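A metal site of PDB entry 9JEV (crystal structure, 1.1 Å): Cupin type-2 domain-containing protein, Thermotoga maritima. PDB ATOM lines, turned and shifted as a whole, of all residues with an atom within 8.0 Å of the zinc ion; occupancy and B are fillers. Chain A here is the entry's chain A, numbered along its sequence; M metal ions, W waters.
ND1 of His 56 is in hydrogen-bond range of O of Asp 54 (2.9 Å).
O of His 62 sits at hydrogen-bond distance from N of Val 90 (3.0 Å).
A ring nitrogen (ND1) of His 96 lies within hydrogen-bond range of the backbone carbonyl oxygen (O) of Glu 94 (2.8 Å).
A ring nitrogen (ND1) of His 62 is in hydrogen-bond range of OD2 of CSD 110 (3.0 Å).
ND1 of His 58 lies within hydrogen-bond range of O of Trp 60, at 3.0 Å.
The nearest printed residue that does not touch the zinc ion is Phe 98 (5.5 Å).
The zinc ion is bound by a ring nitrogen (NE2) of His 58 (2.1 Å).
The zinc ion is bound by NE2 of His 62.
NE2 of His 96 is bound to the zinc ion, 2.1 Å away.
NE2 of His 56 is bound to the zinc ion (2.2 Å).
Water W1 binds the zinc ion (2.2 Å).
Water W2 is bound to the zinc ion (2.2 Å).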
ATOM      1  N   LYS A  22      21.082 -22.864  -0.150  1.00  0.00           N
ATOM      2  CA  LYS A  22      21.047 -23.832   0.927  1.00  0.00           C
ATOM      3  C   LYS A  22      20.045 -24.963   0.672  1.00  0.00           C
ATOM      4  O   LYS A  22      19.825 -25.761   1.585  1.00  0.00           O
ATOM      5  CB  LYS A  22      20.795 -23.109   2.256  1.00  0.00           C
ATOM      6  CG  LYS A  22      19.532 -22.285   2.393  1.00  0.00           C
ATOM      7  CD  LYS A  22      19.467 -21.568   3.739  1.00  0.00           C
ATOM      8  CE  LYS A  22      18.350 -20.529   3.822  1.00  0.00           C
ATOM      9  NZ  LYS A  22      18.242 -19.931   5.175  1.00  0.00           N
ATOM     10  N   ARG A  43       2.195 -26.519   2.654  1.00  0.00           N
ATOM     11  CA  ARG A  43       3.007 -26.901   1.507  1.00  0.00           C
ATOM     12  C   ARG A  43       3.274 -28.395   1.512  1.00  0.00           C
ATOM     13  O   ARG A  43       3.321 -29.000   2.576  1.00  0.00           O
ATOM     14  CB  ARG A  43       4.345 -26.164   1.526  1.00  0.00           C
ATOM     15  CG  ARG A  43       4.259 -24.659   1.560  1.00  0.00           C
ATOM     16  CD  ARG A  43       4.268 -24.098   2.958  1.00  0.00           C
ATOM     17  NE  ARG A  43       5.485 -24.333   3.740  1.00  0.00           N
ATOM     18  CZ  ARG A  43       6.679 -23.749   3.635  1.00  0.00           C
ATOM     19  NH1 ARG A  43       7.684 -24.078   4.440  1.00  0.00           N
ATOM     20  NH2 ARG A  43       6.905 -22.835   2.720  1.00  0.00           N
ATOM     21  N   PHE A  45       6.285 -30.753   0.170  1.00  0.00           N
ATOM     22  CA  PHE A  45       7.652 -30.790  -0.346  1.00  0.00           C
ATOM     23  C   PHE A  45       7.988 -32.191  -0.847  1.00  0.00           C
ATOM     24  O   PHE A  45       7.618 -33.189  -0.236  1.00  0.00           O
ATOM     25  CB  PHE A  45       8.657 -30.417   0.737  1.00  0.00           C
ATOM     26  CG  PHE A  45       8.758 -28.948   0.985  1.00  0.00           C
ATOM     27  CD1 PHE A  45       9.649 -28.179   0.246  1.00  0.00           C
ATOM     28  CD2 PHE A  45       7.970 -28.315   1.914  1.00  0.00           C
ATOM     29  CE1 PHE A  45       9.729 -26.814   0.454  1.00  0.00           C
ATOM     30  CE2 PHE A  45       8.056 -26.963   2.142  1.00  0.00           C
ATOM     31  CZ  PHE A  45       8.941 -26.199   1.397  1.00  0.00           C
ATOM     32  N   ILE A  53      18.374 -30.071   2.131  1.00  0.00           N
ATOM     33  CA  ILE A  53      18.035 -28.800   2.750  1.00  0.00           C
ATOM     34  C   ILE A  53      19.045 -28.587   3.858  1.00  0.00           C
ATOM     35  O   ILE A  53      18.979 -29.276   4.889  1.00  0.00           O
ATOM     36  CB  ILE A  53      16.593 -28.826   3.245  1.00  0.00           C
ATOM     37  CG1 ILE A  53      15.595 -28.980   2.095  1.00  0.00           C
ATOM     38  CG2 ILE A  53      16.274 -27.609   4.094  1.00  0.00           C
ATOM     39  CD1 ILE A  53      14.191 -29.376   2.509  1.00  0.00           C
ATOM     40  N   ASP A  54      20.019 -27.723   3.617  1.00  0.00           N
ATOM     41  CA  ASP A  54      21.102 -27.525   4.571  1.00  0.00           C
ATOM     42  C   ASP A  54      20.554 -27.048   5.917  1.00  0.00           C
ATOM     43  O   ASP A  54      19.525 -26.399   5.996  1.00  0.00           O
ATOM     44  CB  ASP A  54      22.077 -26.470   4.101  1.00  0.00           C
ATOM     45  CG  ASP A  54      22.856 -26.708   2.858  1.00  0.00           C
ATOM     46  OD1 ASP A  54      22.851 -27.878   2.409  1.00  0.00           O
ATOM     47  OD2 ASP A  54      23.491 -25.741   2.383  1.00  0.00           O
ATOM     48  N   ARG A  55      21.306 -27.359   6.965  1.00  0.00           N
ATOM     49  CA  ARG A  55      20.998 -26.800   8.286  1.00  0.00           C
ATOM     50  C   ARG A  55      20.804 -25.289   8.213  1.00  0.00           C
ATOM     51  O   ARG A  55      21.640 -24.585   7.642  1.00  0.00           O
ATOM     52  CB  ARG A  55      22.113 -27.129   9.273  1.00  0.00           C
ATOM     53  CG  ARG A  55      22.094 -28.586   9.730  1.00  0.00           C
ATOM     54  CD  ARG A  55      23.221 -28.807  10.748  1.00  0.00           C
ATOM     55  NE  ARG A  55      23.152 -30.145  11.303  1.00  0.00           N
ATOM     56  CZ  ARG A  55      23.660 -31.253  10.777  1.00  0.00           C
ATOM     57  NH1 ARG A  55      24.318 -31.214   9.639  1.00  0.00           N
ATOM     58  NH2 ARG A  55      23.493 -32.390  11.428  1.00  0.00           N
ATOM     59  N   HIS A  56      19.752 -24.806   8.828  1.00  0.00           N
ATOM     60  CA  HIS A  56      19.370 -23.405   8.829  1.00  0.00           C
ATOM     61  C   HIS A  56      18.413 -23.170   9.993  1.00  0.00           C
ATOM     62  O   HIS A  56      17.991 -24.108  10.669  1.00  0.00           O
ATOM     63  CB  HIS A  56      18.753 -22.959   7.498  1.00  0.00           C
ATOM     64  CG  HIS A  56      17.406 -23.604   7.305  1.00  0.00           C
ATOM     65  ND1 HIS A  56      17.234 -24.914   6.951  1.00  0.00           N
ATOM     66  CD2 HIS A  56      16.146 -23.112   7.443  1.00  0.00           C
ATOM     67  CE1 HIS A  56      15.931 -25.197   6.878  1.00  0.00           C
ATOM     68  NE2 HIS A  56      15.221 -24.113   7.172  1.00  0.00           N
ATOM     69  N   SER A  57      18.080 -21.916  10.221  1.00  0.00           N
ATOM     70  CA  SER A  57      17.052 -21.571  11.206  1.00  0.00           C
ATOM     71  C   SER A  57      16.331 -20.307  10.734  1.00  0.00           C
ATOM     72  O   SER A  57      16.829 -19.582   9.896  1.00  0.00           O
ATOM     73  CB  SER A  57      17.640 -21.369  12.584  1.00  0.00           C
ATOM     74  OG  SER A  57      18.541 -20.287  12.608  1.00  0.00           O
ATOM     75  N   HIS A  58      15.164 -20.051  11.334  1.00  0.00           N
ATOM     76  CA  HIS A  58      14.368 -18.885  10.994  1.00  0.00           C
ATOM     77  C   HIS A  58      13.451 -18.581  12.174  1.00  0.00           C
ATOM     78  O   HIS A  58      13.158 -19.478  12.966  1.00  0.00           O
ATOM     79  CB  HIS A  58      13.525 -19.026   9.732  1.00  0.00           C
ATOM     80  CG  HIS A  58      13.089 -20.440   9.491  1.00  0.00           C
ATOM     81  ND1 HIS A  58      12.219 -21.135  10.311  1.00  0.00           N
ATOM     82  CD2 HIS A  58      13.469 -21.313   8.537  1.00  0.00           C
ATOM     83  CE1 HIS A  58      12.086 -22.372   9.830  1.00  0.00           C
ATOM     84  NE2 HIS A  58      12.829 -22.516   8.754  1.00  0.00           N
ATOM     85  N   TRP A  60      10.373 -18.554  12.859  1.00  0.00           N
ATOM     86  CA  TRP A  60       9.089 -19.188  12.900  1.00  0.00           C
ATOM     87  C   TRP A  60       9.315 -20.715  13.018  1.00  0.00           C
ATOM     88  O   TRP A  60      10.363 -21.214  12.612  1.00  0.00           O
ATOM     89  CB  TRP A  60       8.237 -18.886  11.666  1.00  0.00           C
ATOM     90  CG  TRP A  60       8.845 -19.202  10.346  1.00  0.00           C
ATOM     91  CD1 TRP A  60       8.836 -20.392   9.695  1.00  0.00           C
ATOM     92  CD2 TRP A  60       9.578 -18.300   9.527  1.00  0.00           C
ATOM     93  NE1 TRP A  60       9.516 -20.286   8.498  1.00  0.00           N
ATOM     94  CE2 TRP A  60       9.979 -19.008   8.376  1.00  0.00           C
ATOM     95  CE3 TRP A  60       9.939 -16.946   9.633  1.00  0.00           C
ATOM     96  CZ2 TRP A  60      10.704 -18.422   7.335  1.00  0.00           C
ATOM     97  CZ3 TRP A  60      10.654 -16.369   8.609  1.00  0.00           C
ATOM     98  CH2 TRP A  60      11.030 -17.088   7.490  1.00  0.00           C
ATOM     99  N   GLU A  61       8.292 -21.383  13.503  1.00  0.00           N
ATOM    100  CA  GLU A  61       8.236 -22.814  13.641  1.00  0.00           C
ATOM    101  C   GLU A  61       7.887 -23.521  12.334  1.00  0.00           C
ATOM    102  O   GLU A  61       7.339 -22.923  11.421  1.00  0.00           O
ATOM    103  CB  GLU A  61       7.191 -23.213  14.684  1.00  0.00           C
ATOM    104  CG  GLU A  61       5.746 -22.939  14.327  1.00  0.00           C
ATOM    105  CD  GLU A  61       5.187 -21.565  14.519  1.00  0.00           C
ATOM    106  OE1 GLU A  61       5.963 -20.592  14.639  1.00  0.00           O
ATOM    107  OE2 GLU A  61       3.946 -21.404  14.517  1.00  0.00           O
ATOM    108  N   HIS A  62       8.152 -24.822  12.334  1.00  0.00           N
ATOM    109  CA  HIS A  62       7.606 -25.735  11.344  1.00  0.00           C
ATOM    110  C   HIS A  62       6.761 -26.811  12.041  1.00  0.00           C
ATOM    111  O   HIS A  62       7.147 -27.314  13.082  1.00  0.00           O
ATOM    112  CB  HIS A  62       8.646 -26.534  10.544  1.00  0.00           C
ATOM    113  CG  HIS A  62       9.504 -25.832   9.571  1.00  0.00           C
ATOM    114  ND1 HIS A  62       9.019 -25.296   8.391  1.00  0.00           N
ATOM    115  CD2 HIS A  62      10.851 -25.619   9.529  1.00  0.00           C
ATOM    116  CE1 HIS A  62      10.019 -24.770   7.706  1.00  0.00           C
ATOM    117  NE2 HIS A  62      11.174 -24.961   8.371  1.00  0.00           N
ATOM    118  N   ILE A  64       5.478 -30.489  10.579  1.00  0.00           N
ATOM    119  CA  ILE A  64       5.723 -31.377   9.433  1.00  0.00           C
ATOM    120  C   ILE A  64       5.052 -32.712   9.640  1.00  0.00           C
ATOM    121  O   ILE A  64       5.040 -33.234  10.776  1.00  0.00           O
ATOM    122  CB  ILE A  64       7.245 -31.540   9.263  1.00  0.00           C
ATOM    123  CG1 ILE A  64       7.878 -30.252   8.732  1.00  0.00           C
ATOM    124  CG2 ILE A  64       7.617 -32.722   8.384  1.00  0.00           C
ATOM    125  CD1 ILE A  64       9.365 -30.136   8.854  1.00  0.00           C
ATOM    126  N   VAL A  90       9.400 -28.296  14.777  1.00  0.00           N
ATOM    127  CA  VAL A  90      10.626 -27.538  14.855  1.00  0.00           C
ATOM    128  C   VAL A  90      10.320 -26.193  15.511  1.00  0.00           C
ATOM    129  O   VAL A  90       9.556 -25.399  14.970  1.00  0.00           O
ATOM    130  CB  VAL A  90      11.287 -27.332  13.488  1.00  0.00           C
ATOM    131  CG1 VAL A  90      12.701 -26.723  13.661  1.00  0.00           C
ATOM    132  CG2 VAL A  90      11.402 -28.610  12.644  1.00  0.00           C
ATOM    133  N   GLU A  94      15.189 -22.979  15.952  1.00  0.00           N
ATOM    134  CA  GLU A  94      15.951 -24.239  16.111  1.00  0.00           C
ATOM    135  C   GLU A  94      16.619 -24.627  14.805  1.00  0.00           C
ATOM    136  O   GLU A  94      16.005 -24.528  13.742  1.00  0.00           O
ATOM    137  CB  GLU A  94      14.958 -25.331  16.533  1.00  0.00           C
ATOM    138  CG  GLU A  94      15.495 -26.688  16.872  1.00  0.00           C
ATOM    139  CD  GLU A  94      14.505 -27.594  17.575  1.00  0.00           C
ATOM    140  OE1 GLU A  94      13.252 -27.556  17.442  1.00  0.00           O
ATOM    141  OE2 GLU A  94      15.002 -28.447  18.354  1.00  0.00           O
ATOM    142  N   ILE A  95      17.881 -25.019  14.873  1.00  0.00           N
ATOM    143  CA  ILE A  95      18.602 -25.465  13.689  1.00  0.00           C
ATOM    144  C   ILE A  95      18.016 -26.775  13.190  1.00  0.00           C
ATOM    145  O   ILE A  95      17.715 -27.718  13.929  1.00  0.00           O
ATOM    146  CB  ILE A  95      20.100 -25.607  14.034  1.00  0.00           C
ATOM    147  CG1 ILE A  95      20.734 -24.225  14.302  1.00  0.00           C
ATOM    148  CG2 ILE A  95      20.866 -26.354  12.978  1.00  0.00           C
ATOM    149  CD1 ILE A  95      22.034 -24.325  15.075  1.00  0.00           C
ATOM    150  N   HIS A  96      17.815 -26.845  11.879  1.00  0.00           N
ATOM    151  CA  HIS A  96      17.239 -28.025  11.255  1.00  0.00           C
ATOM    152  C   HIS A  96      17.612 -28.048   9.786  1.00  0.00           C
ATOM    153  O   HIS A  96      17.871 -27.021   9.165  1.00  0.00           O
ATOM    154  CB  HIS A  96      15.717 -28.032  11.430  1.00  0.00           C
ATOM    155  CG  HIS A  96      15.044 -26.862  10.746  1.00  0.00           C
ATOM    156  ND1 HIS A  96      15.135 -25.592  11.272  1.00  0.00           N
ATOM    157  CD2 HIS A  96      14.316 -26.717   9.628  1.00  0.00           C
ATOM    158  CE1 HIS A  96      14.478 -24.758  10.502  1.00  0.00           C
ATOM    159  NE2 HIS A  96      13.965 -25.396   9.473  1.00  0.00           N
ATOM    160  N   GLY A  97      17.605 -29.233   9.208  1.00  0.00           N
ATOM    161  CA  GLY A  97      17.716 -29.433   7.779  1.00  0.00           C
ATOM    162  C   GLY A  97      17.271 -30.857   7.458  1.00  0.00           C
ATOM    163  O   GLY A  97      16.828 -31.556   8.366  1.00  0.00           O
ATOM    164  N   PHE A  98      17.367 -31.240   6.203  1.00  0.00           N
ATOM    165  CA  PHE A  98      16.838 -32.514   5.734  1.00  0.00           C
ATOM    166  C   PHE A  98      17.680 -33.065   4.595  1.00  0.00           C
ATOM    167  O   PHE A  98      18.258 -32.297   3.839  1.00  0.00           O
ATOM    168  CB  PHE A  98      15.389 -32.380   5.252  1.00  0.00           C
ATOM    169  CG  PHE A  98      14.498 -31.762   6.290  1.00  0.00           C
ATOM    170  CD1 PHE A  98      13.944 -32.512   7.311  1.00  0.00           C
ATOM    171  CD2 PHE A  98      14.275 -30.387   6.224  1.00  0.00           C
ATOM    172  CE1 PHE A  98      13.152 -31.901   8.277  1.00  0.00           C
ATOM    173  CE2 PHE A  98      13.500 -29.780   7.192  1.00  0.00           C
ATOM    174  CZ  PHE A  98      12.957 -30.538   8.209  1.00  0.00           C
ATOM    175  N   CSD A 110       4.421 -29.515   5.138  1.00  0.00           N
ATOM    176  CA  CSD A 110       5.172 -28.547   5.983  1.00  0.00           C
ATOM    177  CB  CSD A 110       6.481 -28.239   5.284  1.00  0.00           C
ATOM    178  SG  CSD A 110       7.610 -27.290   6.323  1.00  0.00           S
ATOM    179  C   CSD A 110       4.295 -27.287   6.077  1.00  0.00           C
ATOM    180  O   CSD A 110       3.951 -26.718   5.039  1.00  0.00           O
ATOM    181  OD1 CSD A 110       8.787 -27.118   5.443  1.00  0.00           O
ATOM    182  OD2 CSD A 110       6.922 -26.023   6.437  1.00  0.00           O
ATOM    183  N   ILE A 112       3.760 -23.558   8.142  1.00  0.00           N
ATOM    184  CA  ILE A 112       4.381 -22.460   8.836  1.00  0.00           C
ATOM    185  C   ILE A 112       3.350 -21.352   9.037  1.00  0.00           C
ATOM    186  O   ILE A 112       2.408 -21.217   8.227  1.00  0.00           O
ATOM    187  CB  ILE A 112       5.602 -21.885   8.092  1.00  0.00           C
ATOM    188  CG1 ILE A 112       5.255 -21.324   6.697  1.00  0.00           C
ATOM    189  CG2 ILE A 112       6.694 -22.934   8.040  1.00  0.00           C
ATOM    190  CD1 ILE A 112       6.418 -20.655   5.999  1.00  0.00           C
HETATM  191 ZN    ZN M   1      13.134 -24.375   7.801  1.00  0.00          ZN
HETATM  192  O   HOH W   1      13.207 -26.118   6.438  1.00  0.00           O
HETATM  193  O   HOH W   2      12.455 -23.342   5.958  1.00  0.00           O
